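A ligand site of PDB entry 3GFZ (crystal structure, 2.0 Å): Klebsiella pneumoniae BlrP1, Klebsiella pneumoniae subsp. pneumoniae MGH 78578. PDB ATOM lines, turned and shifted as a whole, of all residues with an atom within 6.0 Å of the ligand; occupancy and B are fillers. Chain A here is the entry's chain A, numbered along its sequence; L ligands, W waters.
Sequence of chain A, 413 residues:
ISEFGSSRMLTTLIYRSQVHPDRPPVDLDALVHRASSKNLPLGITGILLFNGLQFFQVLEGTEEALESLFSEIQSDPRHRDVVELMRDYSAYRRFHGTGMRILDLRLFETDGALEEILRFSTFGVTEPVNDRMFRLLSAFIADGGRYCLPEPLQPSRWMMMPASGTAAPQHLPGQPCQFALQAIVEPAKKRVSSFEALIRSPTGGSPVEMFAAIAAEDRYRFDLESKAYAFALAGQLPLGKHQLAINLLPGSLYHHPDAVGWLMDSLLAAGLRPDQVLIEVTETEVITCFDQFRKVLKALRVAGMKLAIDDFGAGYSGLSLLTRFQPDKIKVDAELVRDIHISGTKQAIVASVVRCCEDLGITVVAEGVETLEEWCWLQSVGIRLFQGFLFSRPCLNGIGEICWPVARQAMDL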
ATOM      1  N   TYR A  15       0.809 -20.645  -3.591  1.00  0.00           N
ATOM      2  CA  TYR A  15       1.670 -21.724  -4.049  1.00  0.00           C
ATOM      3  C   TYR A  15       2.681 -21.165  -5.025  1.00  0.00           C
ATOM      4  O   TYR A  15       2.508 -20.058  -5.544  1.00  0.00           O
ATOM      5  CB  TYR A  15       0.842 -22.853  -4.678  1.00  0.00           C
ATOM      6  CG  TYR A  15       0.250 -22.519  -6.019  1.00  0.00           C
ATOM      7  CD1 TYR A  15       1.000 -22.631  -7.188  1.00  0.00           C
ATOM      8  CD2 TYR A  15      -1.055 -22.051  -6.118  1.00  0.00           C
ATOM      9  CE1 TYR A  15       0.471 -22.312  -8.401  1.00  0.00           C
ATOM     10  CE2 TYR A  15      -1.590 -21.733  -7.344  1.00  0.00           C
ATOM     11  CZ  TYR A  15      -0.822 -21.855  -8.480  1.00  0.00           C
ATOM     12  OH  TYR A  15      -1.334 -21.530  -9.710  1.00  0.00           O
ATOM     13  N   SER A  17       4.948 -22.793  -8.512  1.00  0.00           N
ATOM     14  CA  SER A  17       5.009 -23.917  -9.451  1.00  0.00           C
ATOM     15  C   SER A  17       6.084 -23.675 -10.491  1.00  0.00           C
ATOM     16  O   SER A  17       6.751 -22.632 -10.461  1.00  0.00           O
ATOM     17  CB  SER A  17       3.641 -24.160 -10.098  1.00  0.00           C
ATOM     18  OG  SER A  17       3.352 -23.194 -11.100  1.00  0.00           O
ATOM     19  N   LEU A  31      -4.711 -17.540 -20.467  1.00  0.00           N
ATOM     20  CA  LEU A  31      -4.884 -18.185 -19.167  1.00  0.00           C
ATOM     21  C   LEU A  31      -5.416 -17.195 -18.130  1.00  0.00           C
ATOM     22  O   LEU A  31      -6.412 -17.460 -17.471  1.00  0.00           O
ATOM     23  CB  LEU A  31      -3.552 -18.780 -18.697  1.00  0.00           C
ATOM     24  CG  LEU A  31      -3.543 -19.693 -17.472  1.00  0.00           C
ATOM     25  CD1 LEU A  31      -2.509 -20.781 -17.666  1.00  0.00           C
ATOM     26  CD2 LEU A  31      -3.275 -18.935 -16.178  1.00  0.00           C
ATOM     27  N   ARG A  34      -8.981 -15.657 -18.795  1.00  0.00           N
ATOM     28  CA  ARG A  34      -9.956 -16.704 -18.499  1.00  0.00           C
ATOM     29  C   ARG A  34     -10.050 -16.905 -16.992  1.00  0.00           C
ATOM     30  O   ARG A  34     -11.151 -17.012 -16.466  1.00  0.00           O
ATOM     31  CB  ARG A  34      -9.555 -18.016 -19.186  1.00  0.00           C
ATOM     32  CG  ARG A  34     -10.713 -18.950 -19.454  1.00  0.00           C
ATOM     33  CD  ARG A  34     -10.269 -20.235 -20.155  1.00  0.00           C
ATOM     34  NE  ARG A  34     -11.414 -21.122 -20.409  1.00  0.00           N
ATOM     35  CZ  ARG A  34     -12.049 -21.258 -21.580  1.00  0.00           C
ATOM     36  NH1 ARG A  34     -11.696 -20.559 -22.664  1.00  0.00           N
ATOM     37  NH2 ARG A  34     -13.069 -22.111 -21.660  1.00  0.00           N
ATOM     38  N   ALA A  35      -8.903 -16.952 -16.323  1.00  0.00           N
ATOM     39  CA  ALA A  35      -8.856 -17.067 -14.873  1.00  0.00           C
ATOM     40  C   ALA A  35      -9.638 -15.964 -14.165  1.00  0.00           C
ATOM     41  O   ALA A  35     -10.482 -16.241 -13.325  1.00  0.00           O
ATOM     42  CB  ALA A  35      -7.409 -17.070 -14.388  1.00  0.00           C
ATOM     43  N   SER A  36      -9.351 -14.728 -14.549  1.00  0.00           N
ATOM     44  CA  SER A  36      -9.963 -13.536 -13.958  1.00  0.00           C
ATOM     45  C   SER A  36     -11.479 -13.508 -14.083  1.00  0.00           C
ATOM     46  O   SER A  36     -12.193 -13.248 -13.107  1.00  0.00           O
ATOM     47  CB  SER A  36      -9.379 -12.284 -14.608  1.00  0.00           C
ATOM     48  OG  SER A  36      -9.758 -11.126 -13.890  1.00  0.00           O
ATOM     49  N   LYS A  38     -13.439 -16.069 -14.598  1.00  0.00           N
ATOM     50  CA  LYS A  38     -14.031 -17.182 -13.860  1.00  0.00           C
ATOM     51  C   LYS A  38     -13.982 -16.934 -12.357  1.00  0.00           C
ATOM     52  O   LYS A  38     -14.938 -17.227 -11.636  1.00  0.00           O
ATOM     53  CB  LYS A  38     -13.293 -18.491 -14.181  1.00  0.00           C
ATOM     54  CG  LYS A  38     -13.948 -19.765 -13.645  1.00  0.00           C
ATOM     55  CD  LYS A  38     -13.243 -20.994 -14.214  1.00  0.00           C
ATOM     56  CE  LYS A  38     -13.563 -22.287 -13.458  1.00  0.00           C
ATOM     57  NZ  LYS A  38     -12.390 -23.202 -13.408  1.00  0.00           N
ATOM     58  N   ASN A  39     -12.863 -16.384 -11.888  1.00  0.00           N
ATOM     59  CA  ASN A  39     -12.636 -16.154 -10.452  1.00  0.00           C
ATOM     60  C   ASN A  39     -13.574 -15.163  -9.803  1.00  0.00           C
ATOM     61  O   ASN A  39     -14.088 -15.419  -8.714  1.00  0.00           O
ATOM     62  CB  ASN A  39     -11.218 -15.630 -10.201  1.00  0.00           C
ATOM     63  CG  ASN A  39     -10.172 -16.694 -10.269  1.00  0.00           C
ATOM     64  OD1 ASN A  39     -10.475 -17.866 -10.531  1.00  0.00           O
ATOM     65  ND2 ASN A  39      -8.919 -16.316 -10.039  1.00  0.00           N
ATOM     66  N   ILE A  44     -13.432 -14.976  -5.881  1.00  0.00           N
ATOM     67  CA  ILE A  44     -12.006 -15.309  -5.841  1.00  0.00           C
ATOM     68  C   ILE A  44     -11.233 -14.163  -6.464  1.00  0.00           C
ATOM     69  O   ILE A  44     -11.604 -13.653  -7.522  1.00  0.00           O
ATOM     70  CB  ILE A  44     -11.678 -16.622  -6.588  1.00  0.00           C
ATOM     71  CG1 ILE A  44     -12.370 -17.815  -5.906  1.00  0.00           C
ATOM     72  CG2 ILE A  44     -10.157 -16.860  -6.631  1.00  0.00           C
ATOM     73  CD1 ILE A  44     -12.327 -19.106  -6.716  1.00  0.00           C
ATOM     74  N   LEU A  48      -0.872 -13.417 -10.152  1.00  0.00           N
ATOM     75  CA  LEU A  48       0.047 -14.422 -10.642  1.00  0.00           C
ATOM     76  C   LEU A  48       1.364 -13.737 -10.973  1.00  0.00           C
ATOM     77  O   LEU A  48       1.393 -12.792 -11.748  1.00  0.00           O
ATOM     78  CB  LEU A  48      -0.524 -15.115 -11.892  1.00  0.00           C
ATOM     79  CG  LEU A  48       0.346 -16.169 -12.606  1.00  0.00           C
ATOM     80  CD1 LEU A  48       0.740 -17.281 -11.667  1.00  0.00           C
ATOM     81  CD2 LEU A  48      -0.361 -16.752 -13.838  1.00  0.00           C
ATOM     82  N   PHE A  55       6.008 -19.989 -11.521  1.00  0.00           N
ATOM     83  CA  PHE A  55       4.804 -19.242 -11.185  1.00  0.00           C
ATOM     84  C   PHE A  55       4.712 -19.117  -9.677  1.00  0.00           C
ATOM     85  O   PHE A  55       5.171 -19.999  -8.941  1.00  0.00           O
ATOM     86  CB  PHE A  55       3.551 -19.967 -11.673  1.00  0.00           C
ATOM     87  CG  PHE A  55       3.463 -20.088 -13.166  1.00  0.00           C
ATOM     88  CD1 PHE A  55       3.219 -18.966 -13.950  1.00  0.00           C
ATOM     89  CD2 PHE A  55       3.600 -21.316 -13.804  1.00  0.00           C
ATOM     90  CE1 PHE A  55       3.144 -19.064 -15.317  1.00  0.00           C
ATOM     91  CE2 PHE A  55       3.516 -21.419 -15.175  1.00  0.00           C
ATOM     92  CZ  PHE A  55       3.298 -20.298 -15.932  1.00  0.00           C
ATOM     93  N   GLN A  57       1.409 -17.886  -7.234  1.00  0.00           N
ATOM     94  CA  GLN A  57       0.021 -17.404  -7.262  1.00  0.00           C
ATOM     95  C   GLN A  57      -0.518 -17.258  -5.859  1.00  0.00           C
ATOM     96  O   GLN A  57      -0.308 -18.104  -5.015  1.00  0.00           O
ATOM     97  CB  GLN A  57      -0.874 -18.345  -8.061  1.00  0.00           C
ATOM     98  CG  GLN A  57      -2.231 -17.708  -8.436  1.00  0.00           C
ATOM     99  CD  GLN A  57      -3.038 -18.527  -9.418  1.00  0.00           C
ATOM    100  OE1 GLN A  57      -3.167 -19.739  -9.274  1.00  0.00           O
ATOM    101  NE2 GLN A  57      -3.575 -17.862 -10.431  1.00  0.00           N
ATOM    102  N   LEU A  59      -4.175 -16.647  -4.005  1.00  0.00           N
ATOM    103  CA  LEU A  59      -5.605 -16.765  -4.208  1.00  0.00           C
ATOM    104  C   LEU A  59      -6.310 -16.423  -2.920  1.00  0.00           C
ATOM    105  O   LEU A  59      -5.819 -16.756  -1.845  1.00  0.00           O
ATOM    106  CB  LEU A  59      -5.988 -18.186  -4.652  1.00  0.00           C
ATOM    107  CG  LEU A  59      -5.514 -18.572  -6.070  1.00  0.00           C
ATOM    108  CD1 LEU A  59      -5.633 -20.056  -6.305  1.00  0.00           C
ATOM    109  CD2 LEU A  59      -6.298 -17.805  -7.124  1.00  0.00           C
ATOM    110  N   LEU A  69     -10.833 -24.802  -6.640  1.00  0.00           N
ATOM    111  CA  LEU A  69      -9.973 -24.231  -7.672  1.00  0.00           C
ATOM    112  C   LEU A  69      -8.570 -24.830  -7.619  1.00  0.00           C
ATOM    113  O   LEU A  69      -8.075 -25.351  -8.615  1.00  0.00           O
ATOM    114  CB  LEU A  69      -9.910 -22.709  -7.531  1.00  0.00           C
ATOM    115  CG  LEU A  69      -8.890 -21.984  -8.413  1.00  0.00           C
ATOM    116  CD1 LEU A  69      -9.118 -22.338  -9.887  1.00  0.00           C
ATOM    117  CD2 LEU A  69      -8.990 -20.489  -8.202  1.00  0.00           C
ATOM    118  N   GLU A  72      -8.173 -28.058  -9.269  1.00  0.00           N
ATOM    119  CA  GLU A  72      -8.069 -27.987 -10.725  1.00  0.00           C
ATOM    120  C   GLU A  72      -6.651 -27.572 -11.124  1.00  0.00           C
ATOM    121  O   GLU A  72      -6.076 -28.140 -12.061  1.00  0.00           O
ATOM    122  CB  GLU A  72      -9.071 -26.989 -11.323  1.00  0.00           C
ATOM    123  CG  GLU A  72     -10.537 -27.412 -11.230  1.00  0.00           C
ATOM    124  CD  GLU A  72     -11.481 -26.451 -11.971  1.00  0.00           C
ATOM    125  OE1 GLU A  72     -11.578 -25.272 -11.574  1.00  0.00           O
ATOM    126  OE2 GLU A  72     -12.115 -26.875 -12.967  1.00  0.00           O
ATOM    127  N   ILE A  73      -6.098 -26.579 -10.418  1.00  0.00           N
ATOM    128  CA  ILE A  73      -4.768 -26.057 -10.713  1.00  0.00           C
ATOM    129  C   ILE A  73      -3.674 -27.093 -10.500  1.00  0.00           C
ATOM    130  O   ILE A  73      -2.797 -27.236 -11.334  1.00  0.00           O
ATOM    131  CB  ILE A  73      -4.439 -24.801  -9.865  1.00  0.00           C
ATOM    132  CG1 ILE A  73      -5.299 -23.614 -10.300  1.00  0.00           C
ATOM    133  CG2 ILE A  73      -2.958 -24.439  -9.984  1.00  0.00           C
ATOM    134  CD1 ILE A  73      -5.361 -22.465  -9.315  1.00  0.00           C
ATOM    135  N   GLN A  74      -3.734 -27.827  -9.380  1.00  0.00           N
ATOM    136  CA  GLN A  74      -2.792 -28.908  -9.092  1.00  0.00           C
ATOM    137  C   GLN A  74      -2.724 -29.970 -10.203  1.00  0.00           C
ATOM    138  O   GLN A  74      -1.674 -30.574 -10.430  1.00  0.00           O
ATOM    139  CB  GLN A  74      -3.161 -29.613  -7.789  1.00  0.00           C
ATOM    140  CG  GLN A  74      -2.679 -28.941  -6.543  1.00  0.00           C
ATOM    141  CD  GLN A  74      -3.055 -29.725  -5.302  1.00  0.00           C
ATOM    142  OE1 GLN A  74      -4.231 -29.856  -4.982  1.00  0.00           O
ATOM    143  NE2 GLN A  74      -2.051 -30.253  -4.611  1.00  0.00           N
ATOM    144  N   ASP A  76      -3.429 -29.308 -13.432  1.00  0.00           N
ATOM    145  CA  ASP A  76      -3.266 -28.673 -14.727  1.00  0.00           C
ATOM    146  C   ASP A  76      -1.924 -29.110 -15.361  1.00  0.00           C
ATOM    147  O   ASP A  76      -0.871 -28.964 -14.740  1.00  0.00           O
ATOM    148  CB  ASP A  76      -3.309 -27.154 -14.607  1.00  0.00           C
ATOM    149  CG  ASP A  76      -3.568 -26.473 -15.933  1.00  0.00           C
ATOM    150  OD1 ASP A  76      -2.803 -26.714 -16.880  1.00  0.00           O
ATOM    151  OD2 ASP A  76      -4.534 -25.691 -16.033  1.00  0.00           O
ATOM    152  N   ARG A  78      -0.232 -27.663 -17.597  1.00  0.00           N
ATOM    153  CA  ARG A  78       0.589 -26.506 -17.968  1.00  0.00           C
ATOM    154  C   ARG A  78       1.735 -26.189 -17.011  1.00  0.00           C
ATOM    155  O   ARG A  78       2.580 -25.342 -17.325  1.00  0.00           O
ATOM    156  CB  ARG A  78      -0.289 -25.258 -18.062  1.00  0.00           C
ATOM    157  CG  ARG A  78      -1.307 -25.278 -19.179  1.00  0.00           C
ATOM    158  CD  ARG A  78      -2.162 -24.039 -19.025  1.00  0.00           C
ATOM    159  NE  ARG A  78      -3.324 -24.036 -19.887  1.00  0.00           N
ATOM    160  CZ  ARG A  78      -4.600 -23.924 -19.489  1.00  0.00           C
ATOM    161  NH1 ARG A  78      -4.940 -23.826 -18.208  1.00  0.00           N
ATOM    162  NH2 ARG A  78      -5.557 -23.939 -20.424  1.00  0.00           N
ATOM    163  N   HIS A  79       1.763 -26.836 -15.844  1.00  0.00           N
ATOM    164  CA  HIS A  79       2.840 -26.644 -14.892  1.00  0.00           C
ATOM    165  C   HIS A  79       3.042 -27.912 -14.063  1.00  0.00           C
ATOM    166  O   HIS A  79       2.298 -28.883 -14.218  1.00  0.00           O
ATOM    167  CB  HIS A  79       2.608 -25.379 -14.039  1.00  0.00           C
ATOM    168  CG  HIS A  79       1.410 -25.449 -13.141  1.00  0.00           C
ATOM    169  ND1 HIS A  79       1.197 -24.514 -12.141  1.00  0.00           N
ATOM    170  CD2 HIS A  79       0.372 -26.315 -13.062  1.00  0.00           C
ATOM    171  CE1 HIS A  79       0.083 -24.808 -11.494  1.00  0.00           C
ATOM    172  NE2 HIS A  79      -0.450 -25.888 -12.046  1.00  0.00           N
ATOM    173  N   GLY A  99      -9.816 -10.313 -10.331  1.00  0.00           N
ATOM    174  CA  GLY A  99     -10.082 -11.742 -10.453  1.00  0.00           C
ATOM    175  C   GLY A  99      -8.785 -12.509 -10.534  1.00  0.00           C
ATOM    176  O   GLY A  99      -8.552 -13.443  -9.773  1.00  0.00           O
ATOM    177  N   MET A 100      -7.956 -12.123 -11.491  1.00  0.00           N
ATOM    178  CA  MET A 100      -6.594 -12.584 -11.593  1.00  0.00           C
ATOM    179  C   MET A 100      -5.838 -11.632 -12.492  1.00  0.00           C
ATOM    180  O   MET A 100      -6.417 -11.005 -13.374  1.00  0.00           O
ATOM    181  CB  MET A 100      -6.509 -14.001 -12.163  1.00  0.00           C
ATOM    182  CG  MET A 100      -5.104 -14.628 -12.101  1.00  0.00           C
ATOM    183  SD  MET A 100      -4.316 -14.511 -10.483  1.00  0.00           S
ATOM    184  CE  MET A 100      -5.507 -15.349  -9.449  1.00  0.00           C
HETATM  185  N1  LIG L   1      -8.046 -21.240 -13.271  1.00  0.00           N
HETATM  186  C1  LIG L   1      -8.944 -20.421 -12.653  1.00  0.00           C
HETATM  187  O1  LIG L   1     -10.134 -20.609 -12.847  1.00  0.00           O
HETATM  188  N2  LIG L   1      -8.511 -19.391 -11.839  1.00  0.00           N
HETATM  189  C2  LIG L   1      -7.152 -19.225 -11.637  1.00  0.00           C
HETATM  190  O2  LIG L   1      -6.804 -18.486 -10.731  1.00  0.00           O
HETATM  191  C3  LIG L   1      -6.240 -20.063 -12.284  1.00  0.00           C
HETATM  192  N3  LIG L   1      -4.871 -19.904 -12.117  1.00  0.00           N
HETATM  193  C4  LIG L   1      -3.981 -20.745 -12.769  1.00  0.00           C
HETATM  194  C5  LIG L   1      -2.610 -20.561 -12.590  1.00  0.00           C
HETATM  195  C6  LIG L   1      -1.692 -21.398 -13.224  1.00  0.00           C
HETATM  196  C7  LIG L   1      -0.226 -21.061 -13.100  1.00  0.00           C
HETATM  197  C8  LIG L   1      -2.166 -22.422 -14.043  1.00  0.00           C
HETATM  198  C9  LIG L   1      -1.251 -23.346 -14.787  1.00  0.00           C
HETATM  199  C10 LIG L   1      -3.539 -22.610 -14.213  1.00  0.00           C
HETATM  200  C11 LIG L   1      -4.456 -21.769 -13.588  1.00  0.00           C
HETATM  201  N4  LIG L   1      -5.825 -21.940 -13.761  1.00  0.00           N
HETATM  202  C12 LIG L   1      -6.692 -21.079 -13.106  1.00  0.00           C
HETATM  203  C13 LIG L   1      -6.428 -22.809 -14.843  1.00  0.00           C
HETATM  204  C14 LIG L   1      -6.969 -24.092 -14.234  1.00  0.00           C
HETATM  205  O3  LIG L   1      -5.890 -24.949 -13.948  1.00  0.00           O
HETATM  206  C15 LIG L   1      -7.964 -24.825 -15.141  1.00  0.00           C
HETATM  207  O4  LIG L   1      -7.306 -25.094 -16.357  1.00  0.00           O
HETATM  208  C16 LIG L   1      -9.258 -24.072 -15.460  1.00  0.00           C
HETATM  209  O5  LIG L   1      -9.713 -23.322 -14.356  1.00  0.00           O
HETATM  210  C17 LIG L   1     -10.358 -25.031 -15.910  1.00  0.00           C
HETATM  211  O6  LIG L   1     -11.603 -24.373 -15.939  1.00  0.00           O
HETATM  212  P1  LIG L   1     -12.300 -23.901 -17.311  1.00  0.00           P
HETATM  213  O7  LIG L   1     -12.244 -25.018 -18.327  1.00  0.00           O
HETATM  214  O8  LIG L   1     -13.743 -23.500 -17.074  1.00  0.00           O
HETATM  215  O9  LIG L   1     -11.537 -22.694 -17.816  1.00  0.00           O
HETATM  216  O   HOH W   1     -10.086 -20.384 -16.096  1.00  0.00           O
HETATM  217  O   HOH W   2     -11.999 -20.049 -10.863  1.00  0.00           O
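Water W2 bridges the side-chain amide oxygen (OD1) of Asn 39 (2.7 Å) and an oxygen (O1) of the ligand (2.8 Å).
NH1 of Arg 78 is in salt-bridge range of OD2 of Asp 76, 2.9 Å away. The side-chain amide oxygen (OD1) of Asn 39 lies close to the backbone carbonyl oxygen (O) of Ala 35. ND2 of Asn 39 lies within hydrogen-bond range of O of Gly 99. The side-chain carboxylate of Glu 72 is in salt-bridge range of the side-chain amino group of Lys 38, at 2.9 Å. The side-chain amide oxygen (OE1) of Gln 57 is in hydrogen-bond range of the side-chain hydroxyl (OH) of Tyr 15, at 2.6 Å. The side-chain amide nitrogen (NE2) of Gln 57 sits close to the side-chain sulfur (SD) of Met 100. SD of Met 100 is in hydrogen-bond range of N of Leu 48. OG of Ser 17 lies within hydrogen-bond range of ND1 of His 79, at 2.7 Å.
The side-chain carboxylate (OD2) of Asp 76 sits at hydrogen-bond distance from an oxygen (O3) of the ligand (2.6 Å). OD1 of Asn 39 lies within hydrogen-bond range of N2 of the ligand, 2.8 Å away. The side-chain amino group (NZ) of Lys 38 is in salt-bridge range of an oxygen (O8) of the ligand, at 3.9 Å. A nitrogen (N3) of the ligand sits at hydrogen-bond distance from the side-chain amide nitrogen (NE2) of Gln 57 (2.9 Å). The guanidinium group (NE) of Arg 34 lies within salt-bridge range of an oxygen (O9) of the ligand (3.0 Å). NH1 of Arg 78 sits at hydrogen-bond distance from O4 of the ligand, at 3.3 Å.
Merely in contact with the ligand: Tyr 15 (3.3 Å), Leu 69 (3.4 Å), Ala 35 (3.5 Å), Ile 73 (3.6 Å), Met 100 (3.6 Å), Leu 59 (3.7 Å), Glu 72 (3.7 Å), His 79 (3.8 Å), Phe 55 (3.8 Å) and Leu 31 (3.9 Å). Of the 22 residues printed, 16 come within 4 Å of the ligand.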
